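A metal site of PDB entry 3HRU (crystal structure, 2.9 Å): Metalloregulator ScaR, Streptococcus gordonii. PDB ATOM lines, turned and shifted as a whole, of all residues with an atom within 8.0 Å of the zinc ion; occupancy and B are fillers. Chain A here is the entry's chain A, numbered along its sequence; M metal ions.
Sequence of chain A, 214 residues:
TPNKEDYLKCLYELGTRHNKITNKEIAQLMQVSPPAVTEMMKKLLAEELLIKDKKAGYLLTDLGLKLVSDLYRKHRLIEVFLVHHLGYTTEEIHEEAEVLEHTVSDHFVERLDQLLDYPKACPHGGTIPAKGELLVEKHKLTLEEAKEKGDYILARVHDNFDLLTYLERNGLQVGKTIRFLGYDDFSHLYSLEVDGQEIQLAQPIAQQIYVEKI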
ATOM      1  N   TYR A  72     -11.135 -26.118 -13.766  1.00  0.00           N
ATOM      2  CA  TYR A  72     -10.530 -25.570 -14.957  1.00  0.00           C
ATOM      3  C   TYR A  72     -11.327 -25.934 -16.207  1.00  0.00           C
ATOM      4  O   TYR A  72     -11.607 -25.044 -17.006  1.00  0.00           O
ATOM      5  CB  TYR A  72      -9.036 -25.939 -15.066  1.00  0.00           C
ATOM      6  CG  TYR A  72      -8.131 -25.116 -14.167  1.00  0.00           C
ATOM      7  CD1 TYR A  72      -6.830 -24.887 -14.515  1.00  0.00           C
ATOM      8  CD2 TYR A  72      -8.590 -24.544 -12.988  1.00  0.00           C
ATOM      9  CE1 TYR A  72      -5.970 -24.129 -13.707  1.00  0.00           C
ATOM     10  CE2 TYR A  72      -7.741 -23.779 -12.175  1.00  0.00           C
ATOM     11  CZ  TYR A  72      -6.425 -23.578 -12.533  1.00  0.00           C
ATOM     12  OH  TYR A  72      -5.563 -22.823 -11.753  1.00  0.00           O
ATOM     13  N   HIS A  75     -14.292 -23.550 -16.079  1.00  0.00           N
ATOM     14  CA  HIS A  75     -13.848 -22.179 -16.322  1.00  0.00           C
ATOM     15  C   HIS A  75     -13.459 -21.931 -17.741  1.00  0.00           C
ATOM     16  O   HIS A  75     -13.831 -20.924 -18.323  1.00  0.00           O
ATOM     17  CB  HIS A  75     -12.631 -21.937 -15.459  1.00  0.00           C
ATOM     18  CG  HIS A  75     -12.028 -20.576 -15.638  1.00  0.00           C
ATOM     19  ND1 HIS A  75     -12.440 -19.483 -14.912  1.00  0.00           N
ATOM     20  CD2 HIS A  75     -11.004 -20.151 -16.411  1.00  0.00           C
ATOM     21  CE1 HIS A  75     -11.724 -18.431 -15.246  1.00  0.00           C
ATOM     22  NE2 HIS A  75     -10.846 -18.811 -16.163  1.00  0.00           N
ATOM     23  N   ARG A  76     -12.687 -22.857 -18.313  1.00  0.00           N
ATOM     24  CA  ARG A  76     -12.174 -22.672 -19.659  1.00  0.00           C
ATOM     25  C   ARG A  76     -13.238 -22.886 -20.724  1.00  0.00           C
ATOM     26  O   ARG A  76     -13.339 -22.110 -21.676  1.00  0.00           O
ATOM     27  CB  ARG A  76     -10.968 -23.566 -19.869  1.00  0.00           C
ATOM     28  CG  ARG A  76      -9.943 -23.284 -18.799  1.00  0.00           C
ATOM     29  CD  ARG A  76      -8.507 -23.588 -19.204  1.00  0.00           C
ATOM     30  NE  ARG A  76      -7.552 -22.891 -18.332  1.00  0.00           N
ATOM     31  CZ  ARG A  76      -6.362 -23.380 -17.973  1.00  0.00           C
ATOM     32  NH1 ARG A  76      -5.959 -24.568 -18.413  1.00  0.00           N
ATOM     33  NH2 ARG A  76      -5.586 -22.669 -17.175  1.00  0.00           N
ATOM     34  N   LEU A  77     -14.044 -23.923 -20.556  1.00  0.00           N
ATOM     35  CA  LEU A  77     -15.132 -24.191 -21.483  1.00  0.00           C
ATOM     36  C   LEU A  77     -16.105 -23.019 -21.504  1.00  0.00           C
ATOM     37  O   LEU A  77     -16.473 -22.524 -22.576  1.00  0.00           O
ATOM     38  CB  LEU A  77     -15.852 -25.468 -21.101  1.00  0.00           C
ATOM     39  CG  LEU A  77     -15.183 -26.801 -21.463  1.00  0.00           C
ATOM     40  CD1 LEU A  77     -16.144 -27.948 -21.199  1.00  0.00           C
ATOM     41  CD2 LEU A  77     -14.811 -26.795 -22.913  1.00  0.00           C
ATOM     42  N   GLU A  79     -15.481 -20.043 -20.772  1.00  0.00           N
ATOM     43  CA  GLU A  79     -14.759 -18.953 -21.387  1.00  0.00           C
ATOM     44  C   GLU A  79     -14.926 -19.126 -22.889  1.00  0.00           C
ATOM     45  O   GLU A  79     -15.420 -18.221 -23.552  1.00  0.00           O
ATOM     46  CB  GLU A  79     -13.296 -19.009 -20.976  1.00  0.00           C
ATOM     47  CG  GLU A  79     -12.662 -17.639 -20.796  1.00  0.00           C
ATOM     48  CD  GLU A  79     -11.637 -17.623 -19.661  1.00  0.00           C
ATOM     49  OE1 GLU A  79     -10.537 -18.153 -19.904  1.00  0.00           O
ATOM     50  OE2 GLU A  79     -11.915 -17.090 -18.534  1.00  0.00           O
ATOM     51  N   VAL A  80     -14.540 -20.288 -23.412  1.00  0.00           N
ATOM     52  CA  VAL A  80     -14.552 -20.515 -24.861  1.00  0.00           C
ATOM     53  C   VAL A  80     -15.935 -20.297 -25.413  1.00  0.00           C
ATOM     54  O   VAL A  80     -16.104 -19.712 -26.468  1.00  0.00           O
ATOM     55  CB  VAL A  80     -14.263 -21.947 -25.240  1.00  0.00           C
ATOM     56  CG1 VAL A  80     -14.555 -22.153 -26.765  1.00  0.00           C
ATOM     57  CG2 VAL A  80     -12.846 -22.346 -24.825  1.00  0.00           C
ATOM     58  N   VAL A  83     -16.747 -16.248 -25.497  1.00  0.00           N
ATOM     59  CA  VAL A  83     -16.132 -15.411 -26.526  1.00  0.00           C
ATOM     60  C   VAL A  83     -16.337 -15.953 -27.944  1.00  0.00           C
ATOM     61  O   VAL A  83     -16.669 -15.210 -28.863  1.00  0.00           O
ATOM     62  CB  VAL A  83     -14.610 -15.066 -26.252  1.00  0.00           C
ATOM     63  CG1 VAL A  83     -14.129 -15.625 -24.951  1.00  0.00           C
ATOM     64  CG2 VAL A  83     -13.733 -15.526 -27.404  1.00  0.00           C
ATOM     65  N   ILE A  93     -16.368 -10.662 -19.965  1.00  0.00           N
ATOM     66  CA  ILE A  93     -16.047 -11.892 -19.255  1.00  0.00           C
ATOM     67  C   ILE A  93     -15.695 -11.643 -17.799  1.00  0.00           C
ATOM     68  O   ILE A  93     -16.074 -12.414 -16.919  1.00  0.00           O
ATOM     69  CB  ILE A  93     -14.880 -12.593 -19.941  1.00  0.00           C
ATOM     70  CG1 ILE A  93     -15.370 -13.188 -21.250  1.00  0.00           C
ATOM     71  CG2 ILE A  93     -14.303 -13.657 -19.037  1.00  0.00           C
ATOM     72  CD1 ILE A  93     -14.537 -14.331 -21.706  1.00  0.00           C
ATOM     73  N   ALA A 121      -8.263 -26.201 -25.590  1.00  0.00           N
ATOM     74  CA  ALA A 121      -7.623 -25.001 -25.046  1.00  0.00           C
ATOM     75  C   ALA A 121      -8.544 -23.837 -25.063  1.00  0.00           C
ATOM     76  O   ALA A 121      -9.191 -23.558 -26.083  1.00  0.00           O
ATOM     77  CB  ALA A 121      -6.435 -24.645 -25.856  1.00  0.00           C
ATOM     78  N   CYS A 122      -8.583 -23.105 -23.960  1.00  0.00           N
ATOM     79  CA  CYS A 122      -9.382 -21.899 -23.934  1.00  0.00           C
ATOM     80  C   CYS A 122      -8.573 -20.902 -24.733  1.00  0.00           C
ATOM     81  O   CYS A 122      -7.406 -21.184 -25.084  1.00  0.00           O
ATOM     82  CB  CYS A 122      -9.533 -21.429 -22.499  1.00  0.00           C
ATOM     83  SG  CYS A 122      -8.047 -20.698 -21.890  1.00  0.00           S
ATOM     84  N   PRO A 123      -9.151 -19.722 -25.034  1.00  0.00           N
ATOM     85  CA  PRO A 123      -8.433 -18.865 -25.985  1.00  0.00           C
ATOM     86  C   PRO A 123      -7.088 -18.336 -25.436  1.00  0.00           C
ATOM     87  O   PRO A 123      -6.225 -17.910 -26.216  1.00  0.00           O
ATOM     88  CB  PRO A 123      -9.433 -17.721 -26.263  1.00  0.00           C
ATOM     89  CG  PRO A 123     -10.713 -18.098 -25.545  1.00  0.00           C
ATOM     90  CD  PRO A 123     -10.325 -19.053 -24.453  1.00  0.00           C
ATOM     91  N   HIS A 124      -6.902 -18.364 -24.113  1.00  0.00           N
ATOM     92  CA  HIS A 124      -5.652 -17.907 -23.516  1.00  0.00           C
ATOM     93  C   HIS A 124      -4.516 -18.908 -23.410  1.00  0.00           C
ATOM     94  O   HIS A 124      -3.604 -18.676 -22.637  1.00  0.00           O
ATOM     95  CB  HIS A 124      -5.927 -17.392 -22.131  1.00  0.00           C
ATOM     96  CG  HIS A 124      -6.950 -16.316 -22.113  1.00  0.00           C
ATOM     97  ND1 HIS A 124      -8.057 -16.362 -21.308  1.00  0.00           N
ATOM     98  CD2 HIS A 124      -7.037 -15.171 -22.825  1.00  0.00           C
ATOM     99  CE1 HIS A 124      -8.792 -15.278 -21.515  1.00  0.00           C
ATOM    100  NE2 HIS A 124      -8.192 -14.540 -22.431  1.00  0.00           N
ATOM    101  N   GLY A 125      -4.587 -19.999 -24.170  1.00  0.00           N
ATOM    102  CA  GLY A 125      -3.562 -21.030 -24.163  1.00  0.00           C
ATOM    103  C   GLY A 125      -3.750 -22.125 -23.102  1.00  0.00           C
ATOM    104  O   GLY A 125      -3.145 -23.211 -23.192  1.00  0.00           O
ATOM    105  N   GLY A 126      -4.558 -21.806 -22.082  1.00  0.00           N
ATOM    106  CA  GLY A 126      -4.844 -22.717 -20.996  1.00  0.00           C
ATOM    107  C   GLY A 126      -5.485 -23.987 -21.534  1.00  0.00           C
ATOM    108  O   GLY A 126      -6.457 -23.924 -22.294  1.00  0.00           O
ATOM    109  N   THR A 127      -4.944 -25.145 -21.174  1.00  0.00           N
ATOM    110  CA  THR A 127      -5.423 -26.362 -21.817  1.00  0.00           C
ATOM    111  C   THR A 127      -6.640 -26.849 -21.062  1.00  0.00           C
ATOM    112  O   THR A 127      -6.825 -26.495 -19.904  1.00  0.00           O
ATOM    113  CB  THR A 127      -4.305 -27.412 -22.049  1.00  0.00           C
ATOM    114  OG1 THR A 127      -4.647 -28.638 -21.404  1.00  0.00           O
ATOM    115  CG2 THR A 127      -2.995 -26.930 -21.499  1.00  0.00           C
ATOM    116  N   ILE A 128      -7.498 -27.616 -21.748  1.00  0.00           N
ATOM    117  CA  ILE A 128      -8.786 -28.048 -21.218  1.00  0.00           C
ATOM    118  C   ILE A 128      -8.813 -29.569 -21.140  1.00  0.00           C
ATOM    119  O   ILE A 128      -8.960 -30.244 -22.163  1.00  0.00           O
ATOM    120  CB  ILE A 128      -9.953 -27.566 -22.130  1.00  0.00           C
ATOM    121  CG1 ILE A 128     -10.073 -26.049 -22.128  1.00  0.00           C
ATOM    122  CG2 ILE A 128     -11.258 -28.142 -21.668  1.00  0.00           C
ATOM    123  CD1 ILE A 128     -11.170 -25.548 -23.079  1.00  0.00           C
ATOM    124  N   ARG A 156       0.705 -18.953 -24.025  1.00  0.00           N
ATOM    125  CA  ARG A 156      -0.341 -18.898 -22.996  1.00  0.00           C
ATOM    126  C   ARG A 156      -0.187 -17.668 -22.098  1.00  0.00           C
ATOM    127  O   ARG A 156       0.926 -17.137 -21.968  1.00  0.00           O
ATOM    128  CB  ARG A 156      -0.308 -20.171 -22.143  1.00  0.00           C
ATOM    129  CG  ARG A 156      -1.274 -20.140 -20.941  1.00  0.00           C
ATOM    130  CD  ARG A 156      -1.559 -21.524 -20.377  1.00  0.00           C
ATOM    131  NE  ARG A 156      -0.500 -21.942 -19.472  1.00  0.00           N
ATOM    132  CZ  ARG A 156      -0.661 -22.014 -18.162  1.00  0.00           C
ATOM    133  NH1 ARG A 156      -1.843 -21.723 -17.620  1.00  0.00           N
ATOM    134  NH2 ARG A 156       0.364 -22.399 -17.398  1.00  0.00           N
ATOM    135  N   VAL A 157      -1.285 -17.210 -21.499  1.00  0.00           N
ATOM    136  CA  VAL A 157      -1.249 -16.149 -20.490  1.00  0.00           C
ATOM    137  C   VAL A 157      -2.287 -16.483 -19.419  1.00  0.00           C
ATOM    138  O   VAL A 157      -3.173 -17.303 -19.654  1.00  0.00           O
ATOM    139  CB  VAL A 157      -1.557 -14.771 -21.091  1.00  0.00           C
ATOM    140  CG1 VAL A 157      -0.990 -14.644 -22.513  1.00  0.00           C
ATOM    141  CG2 VAL A 157      -3.032 -14.542 -21.111  1.00  0.00           C
ATOM    142  N   HIS A 158      -2.194 -15.878 -18.245  1.00  0.00           N
ATOM    143  CA  HIS A 158      -3.186 -16.160 -17.210  1.00  0.00           C
ATOM    144  C   HIS A 158      -4.442 -15.358 -17.517  1.00  0.00           C
ATOM    145  O   HIS A 158      -4.330 -14.322 -18.130  1.00  0.00           O
ATOM    146  CB  HIS A 158      -2.660 -15.822 -15.804  1.00  0.00           C
ATOM    147  CG  HIS A 158      -1.717 -16.852 -15.235  1.00  0.00           C
ATOM    148  ND1 HIS A 158      -2.017 -18.197 -15.209  1.00  0.00           N
ATOM    149  CD2 HIS A 158      -0.516 -16.716 -14.643  1.00  0.00           C
ATOM    150  CE1 HIS A 158      -1.012 -18.855 -14.645  1.00  0.00           C
ATOM    151  NE2 HIS A 158      -0.082 -17.981 -14.290  1.00  0.00           N
ATOM    152  N   ASP A 159      -5.614 -15.837 -17.108  1.00  0.00           N
ATOM    153  CA  ASP A 159      -6.903 -15.192 -17.361  1.00  0.00           C
ATOM    154  C   ASP A 159      -6.972 -13.845 -16.671  1.00  0.00           C
ATOM    155  O   ASP A 159      -7.522 -12.886 -17.221  1.00  0.00           O
ATOM    156  CB  ASP A 159      -8.034 -16.066 -16.801  1.00  0.00           C
ATOM    157  CG  ASP A 159      -8.293 -17.297 -17.644  1.00  0.00           C
ATOM    158  OD1 ASP A 159      -8.442 -18.413 -17.070  1.00  0.00           O
ATOM    159  OD2 ASP A 159      -8.321 -17.134 -18.886  1.00  0.00           O
ATOM    160  N   ASN A 160      -6.461 -13.821 -15.446  1.00  0.00           N
ATOM    161  CA  ASN A 160      -6.328 -12.616 -14.633  1.00  0.00           C
ATOM    162  C   ASN A 160      -6.611 -11.277 -15.371  1.00  0.00           C
ATOM    163  O   ASN A 160      -5.822 -10.800 -16.197  1.00  0.00           O
ATOM    164  CB  ASN A 160      -4.937 -12.639 -13.996  1.00  0.00           C
ATOM    165  CG  ASN A 160      -4.656 -11.439 -13.127  1.00  0.00           C
ATOM    166  OD1 ASN A 160      -5.590 -10.760 -12.676  1.00  0.00           O
ATOM    167  ND2 ASN A 160      -3.377 -11.149 -12.891  1.00  0.00           N
ATOM    168  N   LEU A 164      -4.538  -9.302 -18.130  1.00  0.00           N
ATOM    169  CA  LEU A 164      -5.062  -9.383 -19.480  1.00  0.00           C
ATOM    170  C   LEU A 164      -5.256  -7.979 -20.037  1.00  0.00           C
ATOM    171  O   LEU A 164      -4.999  -7.711 -21.227  1.00  0.00           O
ATOM    172  CB  LEU A 164      -6.368 -10.153 -19.464  1.00  0.00           C
ATOM    173  CG  LEU A 164      -6.539 -11.254 -20.488  1.00  0.00           C
ATOM    174  CD1 LEU A 164      -5.348 -12.144 -20.500  1.00  0.00           C
ATOM    175  CD2 LEU A 164      -7.764 -12.048 -20.157  1.00  0.00           C
HETATM  176 ZN    ZN M   1      -8.679 -18.744 -20.560  1.00  0.00          ZN
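NE2 of His 75 is in hydrogen-bond range of OE2 of Glu 79 (3.1 Å). A ring nitrogen (NE2) of His 75 lies within hydrogen-bond range of the side-chain carboxylate of Asp 159 (2.6 Å). The backbone carbonyl oxygen (O) of Gly 126 lies close to the side-chain sulfur (SG) of Cys 122 (3.6 Å). O of His 124 lies within hydrogen-bond range of N of Val 157, at 3.0 Å.
Within 4 Å of the zinc ion: Glu 79, Cys 122, His 124 and Asp 159. The nearest printed residue that does not touch the zinc ion is Pro 123 (4.2 Å).
The zinc ion is bound by OE1 of Glu 79, OD2 of Asp 159, SG of Cys 122 and ND1 of His 124. The zinc ion has four donor atoms within binding distance.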
